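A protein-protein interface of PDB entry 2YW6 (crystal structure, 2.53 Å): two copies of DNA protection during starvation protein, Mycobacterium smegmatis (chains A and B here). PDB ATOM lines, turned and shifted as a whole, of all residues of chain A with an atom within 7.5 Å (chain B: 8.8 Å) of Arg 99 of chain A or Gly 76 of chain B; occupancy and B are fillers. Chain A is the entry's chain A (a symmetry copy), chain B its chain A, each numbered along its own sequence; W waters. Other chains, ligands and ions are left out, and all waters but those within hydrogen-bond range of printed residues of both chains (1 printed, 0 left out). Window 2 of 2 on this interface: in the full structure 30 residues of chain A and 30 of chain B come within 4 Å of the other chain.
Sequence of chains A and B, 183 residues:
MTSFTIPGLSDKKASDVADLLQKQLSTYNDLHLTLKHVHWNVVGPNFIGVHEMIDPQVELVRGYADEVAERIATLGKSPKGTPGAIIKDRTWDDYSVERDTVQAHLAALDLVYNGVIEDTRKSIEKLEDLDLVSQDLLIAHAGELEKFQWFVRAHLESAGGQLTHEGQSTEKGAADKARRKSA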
ATOM      1  N   HIS A  37     -12.124  -1.566  -8.409  1.00  0.00           N
ATOM      2  CA  HIS A  37     -11.684  -1.906  -9.750  1.00  0.00           C
ATOM      3  C   HIS A  37     -11.528  -3.429  -9.935  1.00  0.00           C
ATOM      4  O   HIS A  37     -12.002  -3.980 -10.927  1.00  0.00           O
ATOM      5  CB  HIS A  37     -10.352  -1.210 -10.038  1.00  0.00           C
ATOM      6  CG  HIS A  37      -9.748  -1.580 -11.359  1.00  0.00           C
ATOM      7  ND1 HIS A  37      -9.971  -0.860 -12.514  1.00  0.00           N
ATOM      8  CD2 HIS A  37      -8.953  -2.619 -11.709  1.00  0.00           C
ATOM      9  CE1 HIS A  37      -9.343  -1.438 -13.518  1.00  0.00           C
ATOM     10  NE2 HIS A  37      -8.715  -2.509 -13.059  1.00  0.00           N
ATOM     11  N   TRP A  40     -14.821  -5.113 -10.028  1.00  0.00           N
ATOM     12  CA  TRP A  40     -15.482  -4.968 -11.295  1.00  0.00           C
ATOM     13  C   TRP A  40     -14.906  -5.814 -12.415  1.00  0.00           C
ATOM     14  O   TRP A  40     -15.599  -6.098 -13.384  1.00  0.00           O
ATOM     15  CB  TRP A  40     -15.452  -3.506 -11.715  1.00  0.00           C
ATOM     16  CG  TRP A  40     -16.116  -2.595 -10.742  1.00  0.00           C
ATOM     17  CD1 TRP A  40     -17.184  -2.889  -9.932  1.00  0.00           C
ATOM     18  CD2 TRP A  40     -15.824  -1.209 -10.528  1.00  0.00           C
ATOM     19  NE1 TRP A  40     -17.575  -1.768  -9.240  1.00  0.00           N
ATOM     20  CE2 TRP A  40     -16.763  -0.724  -9.588  1.00  0.00           C
ATOM     21  CE3 TRP A  40     -14.869  -0.329 -11.059  1.00  0.00           C
ATOM     22  CZ2 TRP A  40     -16.773   0.610  -9.161  1.00  0.00           C
ATOM     23  CZ3 TRP A  40     -14.881   0.993 -10.642  1.00  0.00           C
ATOM     24  CH2 TRP A  40     -15.829   1.452  -9.698  1.00  0.00           C
ATOM     25  N   ASN A  41     -13.648  -6.224 -12.289  1.00  0.00           N
ATOM     26  CA  ASN A  41     -13.000  -6.986 -13.355  1.00  0.00           C
ATOM     27  C   ASN A  41     -12.596  -8.436 -13.124  1.00  0.00           C
ATOM     28  O   ASN A  41     -11.882  -8.996 -13.948  1.00  0.00           O
ATOM     29  CB  ASN A  41     -11.772  -6.227 -13.843  1.00  0.00           C
ATOM     30  CG  ASN A  41     -12.129  -4.993 -14.617  1.00  0.00           C
ATOM     31  OD1 ASN A  41     -12.025  -3.867 -14.113  1.00  0.00           O
ATOM     32  ND2 ASN A  41     -12.567  -5.191 -15.859  1.00  0.00           N
ATOM     33  N   VAL A  42     -13.012  -9.045 -12.021  1.00  0.00           N
ATOM     34  CA  VAL A  42     -12.666 -10.440 -11.798  1.00  0.00           C
ATOM     35  C   VAL A  42     -13.712 -11.336 -12.462  1.00  0.00           C
ATOM     36  O   VAL A  42     -14.919 -11.131 -12.310  1.00  0.00           O
ATOM     37  CB  VAL A  42     -12.581 -10.813 -10.274  1.00  0.00           C
ATOM     38  CG1 VAL A  42     -11.228 -10.461  -9.727  1.00  0.00           C
ATOM     39  CG2 VAL A  42     -13.666 -10.092  -9.486  1.00  0.00           C
ATOM     40  N   VAL A  43     -13.242 -12.315 -13.221  1.00  0.00           N
ATOM     41  CA  VAL A  43     -14.131 -13.261 -13.875  1.00  0.00           C
ATOM     42  C   VAL A  43     -13.532 -14.612 -13.572  1.00  0.00           C
ATOM     43  O   VAL A  43     -12.418 -14.698 -13.037  1.00  0.00           O
ATOM     44  CB  VAL A  43     -14.212 -13.043 -15.421  1.00  0.00           C
ATOM     45  CG1 VAL A  43     -14.660 -11.609 -15.720  1.00  0.00           C
ATOM     46  CG2 VAL A  43     -12.877 -13.335 -16.078  1.00  0.00           C
ATOM     47  N   SER A  96      -2.693  -1.977 -12.722  1.00  0.00           N
ATOM     48  CA  SER A  96      -2.852  -2.221 -14.151  1.00  0.00           C
ATOM     49  C   SER A  96      -3.519  -3.497 -14.658  1.00  0.00           C
ATOM     50  O   SER A  96      -3.404  -3.803 -15.842  1.00  0.00           O
ATOM     51  CB  SER A  96      -1.485  -2.098 -14.819  1.00  0.00           C
ATOM     52  OG  SER A  96      -0.538  -2.922 -14.167  1.00  0.00           O
ATOM     53  N   VAL A  97      -4.207  -4.245 -13.808  1.00  0.00           N
ATOM     54  CA  VAL A  97      -4.871  -5.458 -14.277  1.00  0.00           C
ATOM     55  C   VAL A  97      -6.318  -5.117 -14.649  1.00  0.00           C
ATOM     56  O   VAL A  97      -7.027  -4.480 -13.867  1.00  0.00           O
ATOM     57  CB  VAL A  97      -4.845  -6.580 -13.187  1.00  0.00           C
ATOM     58  CG1 VAL A  97      -5.455  -7.864 -13.720  1.00  0.00           C
ATOM     59  CG2 VAL A  97      -3.417  -6.853 -12.757  1.00  0.00           C
ATOM     60  N   GLU A  98      -6.735  -5.514 -15.858  1.00  0.00           N
ATOM     61  CA  GLU A  98      -8.097  -5.279 -16.363  1.00  0.00           C
ATOM     62  C   GLU A  98      -8.951  -6.531 -16.199  1.00  0.00           C
ATOM     63  O   GLU A  98      -8.781  -7.269 -15.236  1.00  0.00           O
ATOM     64  CB  GLU A  98      -8.064  -4.886 -17.838  1.00  0.00           C
ATOM     65  CG  GLU A  98      -7.904  -3.401 -18.082  1.00  0.00           C
ATOM     66  CD  GLU A  98      -6.778  -2.797 -17.274  1.00  0.00           C
ATOM     67  OE1 GLU A  98      -5.607  -3.146 -17.534  1.00  0.00           O
ATOM     68  OE2 GLU A  98      -7.059  -1.977 -16.372  1.00  0.00           O
ATOM     69  N   ARG A  99      -9.868  -6.781 -17.130  1.00  0.00           N
ATOM     70  CA  ARG A  99     -10.695  -7.986 -16.999  1.00  0.00           C
ATOM     71  C   ARG A  99      -9.747  -9.179 -16.976  1.00  0.00           C
ATOM     72  O   ARG A  99      -9.020  -9.441 -17.942  1.00  0.00           O
ATOM     73  CB  ARG A  99     -11.698  -8.122 -18.153  1.00  0.00           C
ATOM     74  CG  ARG A  99     -12.548  -9.397 -18.057  1.00  0.00           C
ATOM     75  CD  ARG A  99     -13.690  -9.433 -19.069  1.00  0.00           C
ATOM     76  NE  ARG A  99     -14.757  -8.490 -18.744  1.00  0.00           N
ATOM     77  CZ  ARG A  99     -15.851  -8.306 -19.482  1.00  0.00           C
ATOM     78  NH1 ARG A  99     -16.029  -9.006 -20.598  1.00  0.00           N
ATOM     79  NH2 ARG A  99     -16.768  -7.418 -19.113  1.00  0.00           N
ATOM     80  N   ASP A 100      -9.738  -9.905 -15.871  1.00  0.00           N
ATOM     81  CA  ASP A 100      -8.821 -11.016 -15.776  1.00  0.00           C
ATOM     82  C   ASP A 100      -9.238 -12.011 -14.716  1.00  0.00           C
ATOM     83  O   ASP A 100     -10.147 -11.761 -13.927  1.00  0.00           O
ATOM     84  CB  ASP A 100      -7.414 -10.485 -15.476  1.00  0.00           C
ATOM     85  CG  ASP A 100      -6.324 -11.305 -16.149  1.00  0.00           C
ATOM     86  OD1 ASP A 100      -6.328 -12.545 -15.983  1.00  0.00           O
ATOM     87  OD2 ASP A 100      -5.468 -10.709 -16.837  1.00  0.00           O
ATOM     88  N   THR A 101      -8.549 -13.145 -14.705  1.00  0.00           N
ATOM     89  CA  THR A 101      -8.848 -14.201 -13.769  1.00  0.00           C
ATOM     90  C   THR A 101      -8.670 -13.780 -12.313  1.00  0.00           C
ATOM     91  O   THR A 101      -7.964 -12.820 -11.999  1.00  0.00           O
ATOM     92  CB  THR A 101      -7.957 -15.430 -14.032  1.00  0.00           C
ATOM     93  OG1 THR A 101      -6.580 -15.062 -13.866  1.00  0.00           O
ATOM     94  CG2 THR A 101      -8.179 -15.960 -15.436  1.00  0.00           C
ATOM     95  N   ALA A 104      -5.095 -13.761 -11.404  1.00  0.00           N
ATOM     96  CA  ALA A 104      -4.369 -12.572 -11.826  1.00  0.00           C
ATOM     97  C   ALA A 104      -4.509 -11.376 -10.878  1.00  0.00           C
ATOM     98  O   ALA A 104      -3.515 -10.744 -10.527  1.00  0.00           O
ATOM     99  CB  ALA A 104      -4.809 -12.183 -13.246  1.00  0.00           C
ATOM    100  N   HIS A 105      -5.743 -11.070 -10.469  1.00  0.00           N
ATOM    101  CA  HIS A 105      -6.027  -9.940  -9.571  1.00  0.00           C
ATOM    102  C   HIS A 105      -5.547 -10.197  -8.148  1.00  0.00           C
ATOM    103  O   HIS A 105      -4.944  -9.331  -7.509  1.00  0.00           O
ATOM    104  CB  HIS A 105      -7.535  -9.633  -9.546  1.00  0.00           C
ATOM    105  CG  HIS A 105      -8.060  -9.049 -10.821  1.00  0.00           C
ATOM    106  ND1 HIS A 105      -7.729  -7.778 -11.246  1.00  0.00           N
ATOM    107  CD2 HIS A 105      -8.871  -9.564 -11.773  1.00  0.00           C
ATOM    108  CE1 HIS A 105      -8.319  -7.537 -12.407  1.00  0.00           C
ATOM    109  NE2 HIS A 105      -9.017  -8.606 -12.747  1.00  0.00           N
ATOM    110  N   ASP B  11     -23.032  -4.641 -30.974  1.00  0.00           N
ATOM    111  CA  ASP B  11     -21.660  -4.679 -30.377  1.00  0.00           C
ATOM    112  C   ASP B  11     -20.917  -3.379 -30.683  1.00  0.00           C
ATOM    113  O   ASP B  11     -20.252  -2.813 -29.816  1.00  0.00           O
ATOM    114  CB  ASP B  11     -20.875  -5.875 -30.926  1.00  0.00           C
ATOM    115  CG  ASP B  11     -19.570  -6.082 -30.210  1.00  0.00           C
ATOM    116  OD1 ASP B  11     -18.832  -7.033 -30.544  1.00  0.00           O
ATOM    117  OD2 ASP B  11     -19.288  -5.279 -29.299  1.00  0.00           O
ATOM    118  N   ALA B  14     -22.734  -0.866 -28.895  1.00  0.00           N
ATOM    119  CA  ALA B  14     -22.637  -1.082 -27.463  1.00  0.00           C
ATOM    120  C   ALA B  14     -21.293  -0.564 -26.958  1.00  0.00           C
ATOM    121  O   ALA B  14     -21.148  -0.215 -25.782  1.00  0.00           O
ATOM    122  CB  ALA B  14     -22.789  -2.562 -27.154  1.00  0.00           C
ATOM    123  N   SER B  15     -20.311  -0.524 -27.858  1.00  0.00           N
ATOM    124  CA  SER B  15     -18.981  -0.023 -27.521  1.00  0.00           C
ATOM    125  C   SER B  15     -19.121   1.469 -27.330  1.00  0.00           C
ATOM    126  O   SER B  15     -18.348   2.092 -26.607  1.00  0.00           O
ATOM    127  CB  SER B  15     -17.990  -0.262 -28.658  1.00  0.00           C
ATOM    128  OG  SER B  15     -17.868  -1.637 -28.946  1.00  0.00           O
ATOM    129  N   ALA B  18     -20.558   1.799 -23.843  1.00  0.00           N
ATOM    130  CA  ALA B  18     -19.537   1.499 -22.847  1.00  0.00           C
ATOM    131  C   ALA B  18     -18.587   2.681 -22.685  1.00  0.00           C
ATOM    132  O   ALA B  18     -18.176   3.005 -21.578  1.00  0.00           O
ATOM    133  CB  ALA B  18     -18.766   0.248 -23.244  1.00  0.00           C
ATOM    134  N   ALA B  69     -20.067   0.856 -13.593  1.00  0.00           N
ATOM    135  CA  ALA B  69     -18.960  -0.060 -13.848  1.00  0.00           C
ATOM    136  C   ALA B  69     -19.494  -1.436 -14.220  1.00  0.00           C
ATOM    137  O   ALA B  69     -18.987  -2.085 -15.138  1.00  0.00           O
ATOM    138  CB  ALA B  69     -18.077  -0.168 -12.616  1.00  0.00           C
ATOM    139  N   GLU B  70     -20.519  -1.877 -13.498  1.00  0.00           N
ATOM    140  CA  GLU B  70     -21.116  -3.173 -13.761  1.00  0.00           C
ATOM    141  C   GLU B  70     -21.835  -3.149 -15.096  1.00  0.00           C
ATOM    142  O   GLU B  70     -21.869  -4.148 -15.807  1.00  0.00           O
ATOM    143  CB  GLU B  70     -22.083  -3.544 -12.643  1.00  0.00           C
ATOM    144  CG  GLU B  70     -21.432  -3.472 -11.275  1.00  0.00           C
ATOM    145  CD  GLU B  70     -21.846  -4.592 -10.352  1.00  0.00           C
ATOM    146  OE1 GLU B  70     -23.067  -4.758 -10.113  1.00  0.00           O
ATOM    147  OE2 GLU B  70     -20.941  -5.303  -9.861  1.00  0.00           O
ATOM    148  N   ARG B  71     -22.406  -2.002 -15.438  1.00  0.00           N
ATOM    149  CA  ARG B  71     -23.102  -1.869 -16.704  1.00  0.00           C
ATOM    150  C   ARG B  71     -22.099  -1.982 -17.861  1.00  0.00           C
ATOM    151  O   ARG B  71     -22.406  -2.550 -18.918  1.00  0.00           O
ATOM    152  CB  ARG B  71     -23.844  -0.521 -16.764  1.00  0.00           C
ATOM    153  CG  ARG B  71     -24.752  -0.374 -17.984  1.00  0.00           C
ATOM    154  CD  ARG B  71     -25.783  -1.491 -18.059  1.00  0.00           C
ATOM    155  NE  ARG B  71     -26.491  -1.489 -19.344  1.00  0.00           N
ATOM    156  CZ  ARG B  71     -27.385  -2.401 -19.723  1.00  0.00           C
ATOM    157  NH1 ARG B  71     -27.703  -3.408 -18.922  1.00  0.00           N
ATOM    158  NH2 ARG B  71     -27.948  -2.319 -20.922  1.00  0.00           N
ATOM    159  N   ILE B  72     -20.903  -1.439 -17.648  1.00  0.00           N
ATOM    160  CA  ILE B  72     -19.850  -1.492 -18.652  1.00  0.00           C
ATOM    161  C   ILE B  72     -19.383  -2.939 -18.801  1.00  0.00           C
ATOM    162  O   ILE B  72     -19.187  -3.425 -19.915  1.00  0.00           O
ATOM    163  CB  ILE B  72     -18.659  -0.582 -18.251  1.00  0.00           C
ATOM    164  CG1 ILE B  72     -19.080   0.890 -18.358  1.00  0.00           C
ATOM    165  CG2 ILE B  72     -17.454  -0.873 -19.125  1.00  0.00           C
ATOM    166  CD1 ILE B  72     -18.084   1.885 -17.797  1.00  0.00           C
ATOM    167  N   ALA B  73     -19.212  -3.647 -17.693  1.00  0.00           N
ATOM    168  CA  ALA B  73     -18.774  -5.032 -17.804  1.00  0.00           C
ATOM    169  C   ALA B  73     -19.881  -5.863 -18.451  1.00  0.00           C
ATOM    170  O   ALA B  73     -19.621  -6.818 -19.196  1.00  0.00           O
ATOM    171  CB  ALA B  73     -18.412  -5.589 -16.440  1.00  0.00           C
ATOM    172  N   THR B  74     -21.127  -5.505 -18.181  1.00  0.00           N
ATOM    173  CA  THR B  74     -22.217  -6.251 -18.781  1.00  0.00           C
ATOM    174  C   THR B  74     -22.188  -6.036 -20.288  1.00  0.00           C
ATOM    175  O   THR B  74     -22.454  -6.966 -21.047  1.00  0.00           O
ATOM    176  CB  THR B  74     -23.564  -5.815 -18.199  1.00  0.00           C
ATOM    177  OG1 THR B  74     -23.539  -6.036 -16.782  1.00  0.00           O
ATOM    178  CG2 THR B  74     -24.715  -6.617 -18.815  1.00  0.00           C
ATOM    179  N   LEU B  75     -21.846  -4.819 -20.713  1.00  0.00           N
ATOM    180  CA  LEU B  75     -21.771  -4.483 -22.137  1.00  0.00           C
ATOM    181  C   LEU B  75     -20.508  -5.055 -22.791  1.00  0.00           C
ATOM    182  O   LEU B  75     -20.189  -4.738 -23.939  1.00  0.00           O
ATOM    183  CB  LEU B  75     -21.813  -2.962 -22.342  1.00  0.00           C
ATOM    184  CG  LEU B  75     -23.141  -2.260 -22.051  1.00  0.00           C
ATOM    185  CD1 LEU B  75     -22.940  -0.750 -22.078  1.00  0.00           C
ATOM    186  CD2 LEU B  75     -24.194  -2.701 -23.067  1.00  0.00           C
ATOM    187  N   GLY B  76     -19.780  -5.883 -22.050  1.00  0.00           N
ATOM    188  CA  GLY B  76     -18.590  -6.510 -22.595  1.00  0.00           C
ATOM    189  C   GLY B  76     -17.263  -5.777 -22.489  1.00  0.00           C
ATOM    190  O   GLY B  76     -16.249  -6.264 -23.002  1.00  0.00           O
ATOM    191  N   LYS B  77     -17.245  -4.612 -21.845  1.00  0.00           N
ATOM    192  CA  LYS B  77     -15.999  -3.880 -21.702  1.00  0.00           C
ATOM    193  C   LYS B  77     -15.474  -3.907 -20.276  1.00  0.00           C
ATOM    194  O   LYS B  77     -16.198  -4.245 -19.342  1.00  0.00           O
ATOM    195  CB  LYS B  77     -16.163  -2.444 -22.178  1.00  0.00           C
ATOM    196  CG  LYS B  77     -16.136  -2.326 -23.681  1.00  0.00           C
ATOM    197  CD  LYS B  77     -15.537  -0.999 -24.102  1.00  0.00           C
ATOM    198  CE  LYS B  77     -15.352  -0.931 -25.611  1.00  0.00           C
ATOM    199  NZ  LYS B  77     -14.643   0.306 -26.036  1.00  0.00           N
ATOM    200  N   SER B  78     -14.198  -3.570 -20.124  1.00  0.00           N
ATOM    201  CA  SER B  78     -13.545  -3.550 -18.825  1.00  0.00           C
ATOM    202  C   SER B  78     -13.605  -2.148 -18.227  1.00  0.00           C
ATOM    203  O   SER B  78     -12.939  -1.236 -18.719  1.00  0.00           O
ATOM    204  CB  SER B  78     -12.090  -3.985 -18.978  1.00  0.00           C
ATOM    205  OG  SER B  78     -11.305  -3.538 -17.890  1.00  0.00           O
ATOM    206  N   PRO B  79     -14.418  -1.951 -17.172  1.00  0.00           N
ATOM    207  CA  PRO B  79     -14.536  -0.634 -16.533  1.00  0.00           C
ATOM    208  C   PRO B  79     -13.238  -0.254 -15.808  1.00  0.00           C
ATOM    209  O   PRO B  79     -12.558  -1.108 -15.230  1.00  0.00           O
ATOM    210  CB  PRO B  79     -15.727  -0.805 -15.589  1.00  0.00           C
ATOM    211  CG  PRO B  79     -15.657  -2.267 -15.217  1.00  0.00           C
ATOM    212  CD  PRO B  79     -15.331  -2.927 -16.540  1.00  0.00           C
ATOM    213  N   LYS B  80     -12.893   1.027 -15.849  1.00  0.00           N
ATOM    214  CA  LYS B  80     -11.664   1.514 -15.225  1.00  0.00           C
ATOM    215  C   LYS B  80     -11.956   2.373 -14.003  1.00  0.00           C
ATOM    216  O   LYS B  80     -12.637   3.399 -14.111  1.00  0.00           O
ATOM    217  CB  LYS B  80     -10.854   2.339 -16.240  1.00  0.00           C
ATOM    218  CG  LYS B  80      -9.924   1.546 -17.163  1.00  0.00           C
ATOM    219  CD  LYS B  80     -10.623   0.395 -17.855  1.00  0.00           C
ATOM    220  CE  LYS B  80      -9.698  -0.289 -18.856  1.00  0.00           C
ATOM    221  NZ  LYS B  80      -9.339   0.645 -19.963  1.00  0.00           N
HETATM  222  O   HOH W   1     -19.353  -9.204 -21.564  1.00  0.00           O
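Of the 13 printed residues of chain A, 5 touch a printed residue of chain B. Of the 16 printed residues of chain B, 7 touch a printed residue of chain A. Printed residues of chain B that touch a printed residue of chain A: Ala 69, Ala 73, Gly 76, Lys 77, Ser 78, Pro 79 and Lys 80. Hydrophobic or aromatic side chains of chain B within 4 Å of the printed part of chain A: Ala 69, Ala 73 and Pro 79. Along chain B the printed residues that touch a printed residue of chain A span positions 69 to 80. Among the printed residues, 12 pairs touch across the chains. Among the printed residues, no Asp or Glu carboxylate lies within 4 Å of a Lys or Arg side-chain nitrogen of the other chain.
O of Val 97 of chain A is in hydrogen-bond range of NE2 of His 37 of chain A. The side-chain amide oxygen (OD1) of Asn 41 of chain A sits close to the backbone carbonyl oxygen (O) of His 37 of chain A, 3.2 Å away. The side-chain amide nitrogen of Asn 41 of chain A lies close to the backbone NH of Arg 99 of chain A. The backbone carbonyl oxygen (O) of Ile 72 of chain B sits at hydrogen-bond distance from the backbone NH (N) of Lys 77 of chain B, at 3.0 Å. N of Asp 100 of chain A lies within hydrogen-bond range of O of Asn 41 of chain A (3.0 Å). NE2 of His 105 of chain A is in hydrogen-bond range of O of Glu 98 of chain A, 2.8 Å away.
Printed residues of chain B within 4 Å of Trp 40 of chain A: Ala 69 (3.2 Å) and Pro 79 (3.7 Å). Val 42 of chain A touches none of the printed residues of chain B. Of the printed residues of chain B, Glu 98 of chain A touches Ser 78 and Lys 80. Of the printed residues of chain B, Arg 99 of chain A touches Ala 73 (2.9 Å), Gly 76 (3.7 Å), Lys 77 (3.2 Å) and Ser 78 (3.6 Å). No residue of chain B comes within 4 Å of Asp 100 of chain A. Ser 15 of chain B touches none of the printed residues of chain A. Of chain A, only Arg 99 (3.7 Å) comes within 4 Å of Gly 76 of chain B. The nearest residue of chain B that does not touch Arg 99 of chain A is Ile 72 of chain B (4.7 Å).
No position is printed for both chains.
Water W1 lies within hydrogen-bond range of the backbone carbonyl oxygen (O) of Ala 73 of chain B (3.4 Å), the backbone NH (N) of Gly 76 of chain B (3.4 Å) and the guanidinium group (NH1) of Arg 99 of chain A (3.5 Å).
The guanidinium group (NH2) of Arg 99 of chain A is in hydrogen-bond range of the backbone carbonyl oxygen (O) of Lys 77 of chain B. The backbone carbonyl oxygen (O) of Ala 73 of chain B lies within hydrogen-bond range of the guanidinium group (NH2) of Arg 99 of chain A (2.9 Å). The side-chain amide nitrogen (ND2) of Asn 41 of chain A is in hydrogen-bond range of the side-chain hydroxyl (OG) of Ser 78 of chain B. O of Pro 79 of chain B lies close to OD1 of Asn 41 of chain A, 3.0 Å away.
Among the printed residues, pairs that only touch across the chains: Trp 40 of chain A with Ala 69 of chain B (3.2 Å), Glu 98 of chain A with Ser 78 of chain B (3.4 Å), Arg 99 of chain A with Ser 78 of chain B (3.6 Å), Arg 99 of chain A with Gly 76 of chain B (3.7 Å), His 37 of chain A with Pro 79 of chain B (3.7 Å), Glu 98 of chain A with Lys 80 of chain B (3.7 Å), Trp 40 of chain A with Pro 79 of chain B (3.7 Å) and His 37 of chain A with Lys 80 of chain B (3.98 Å).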
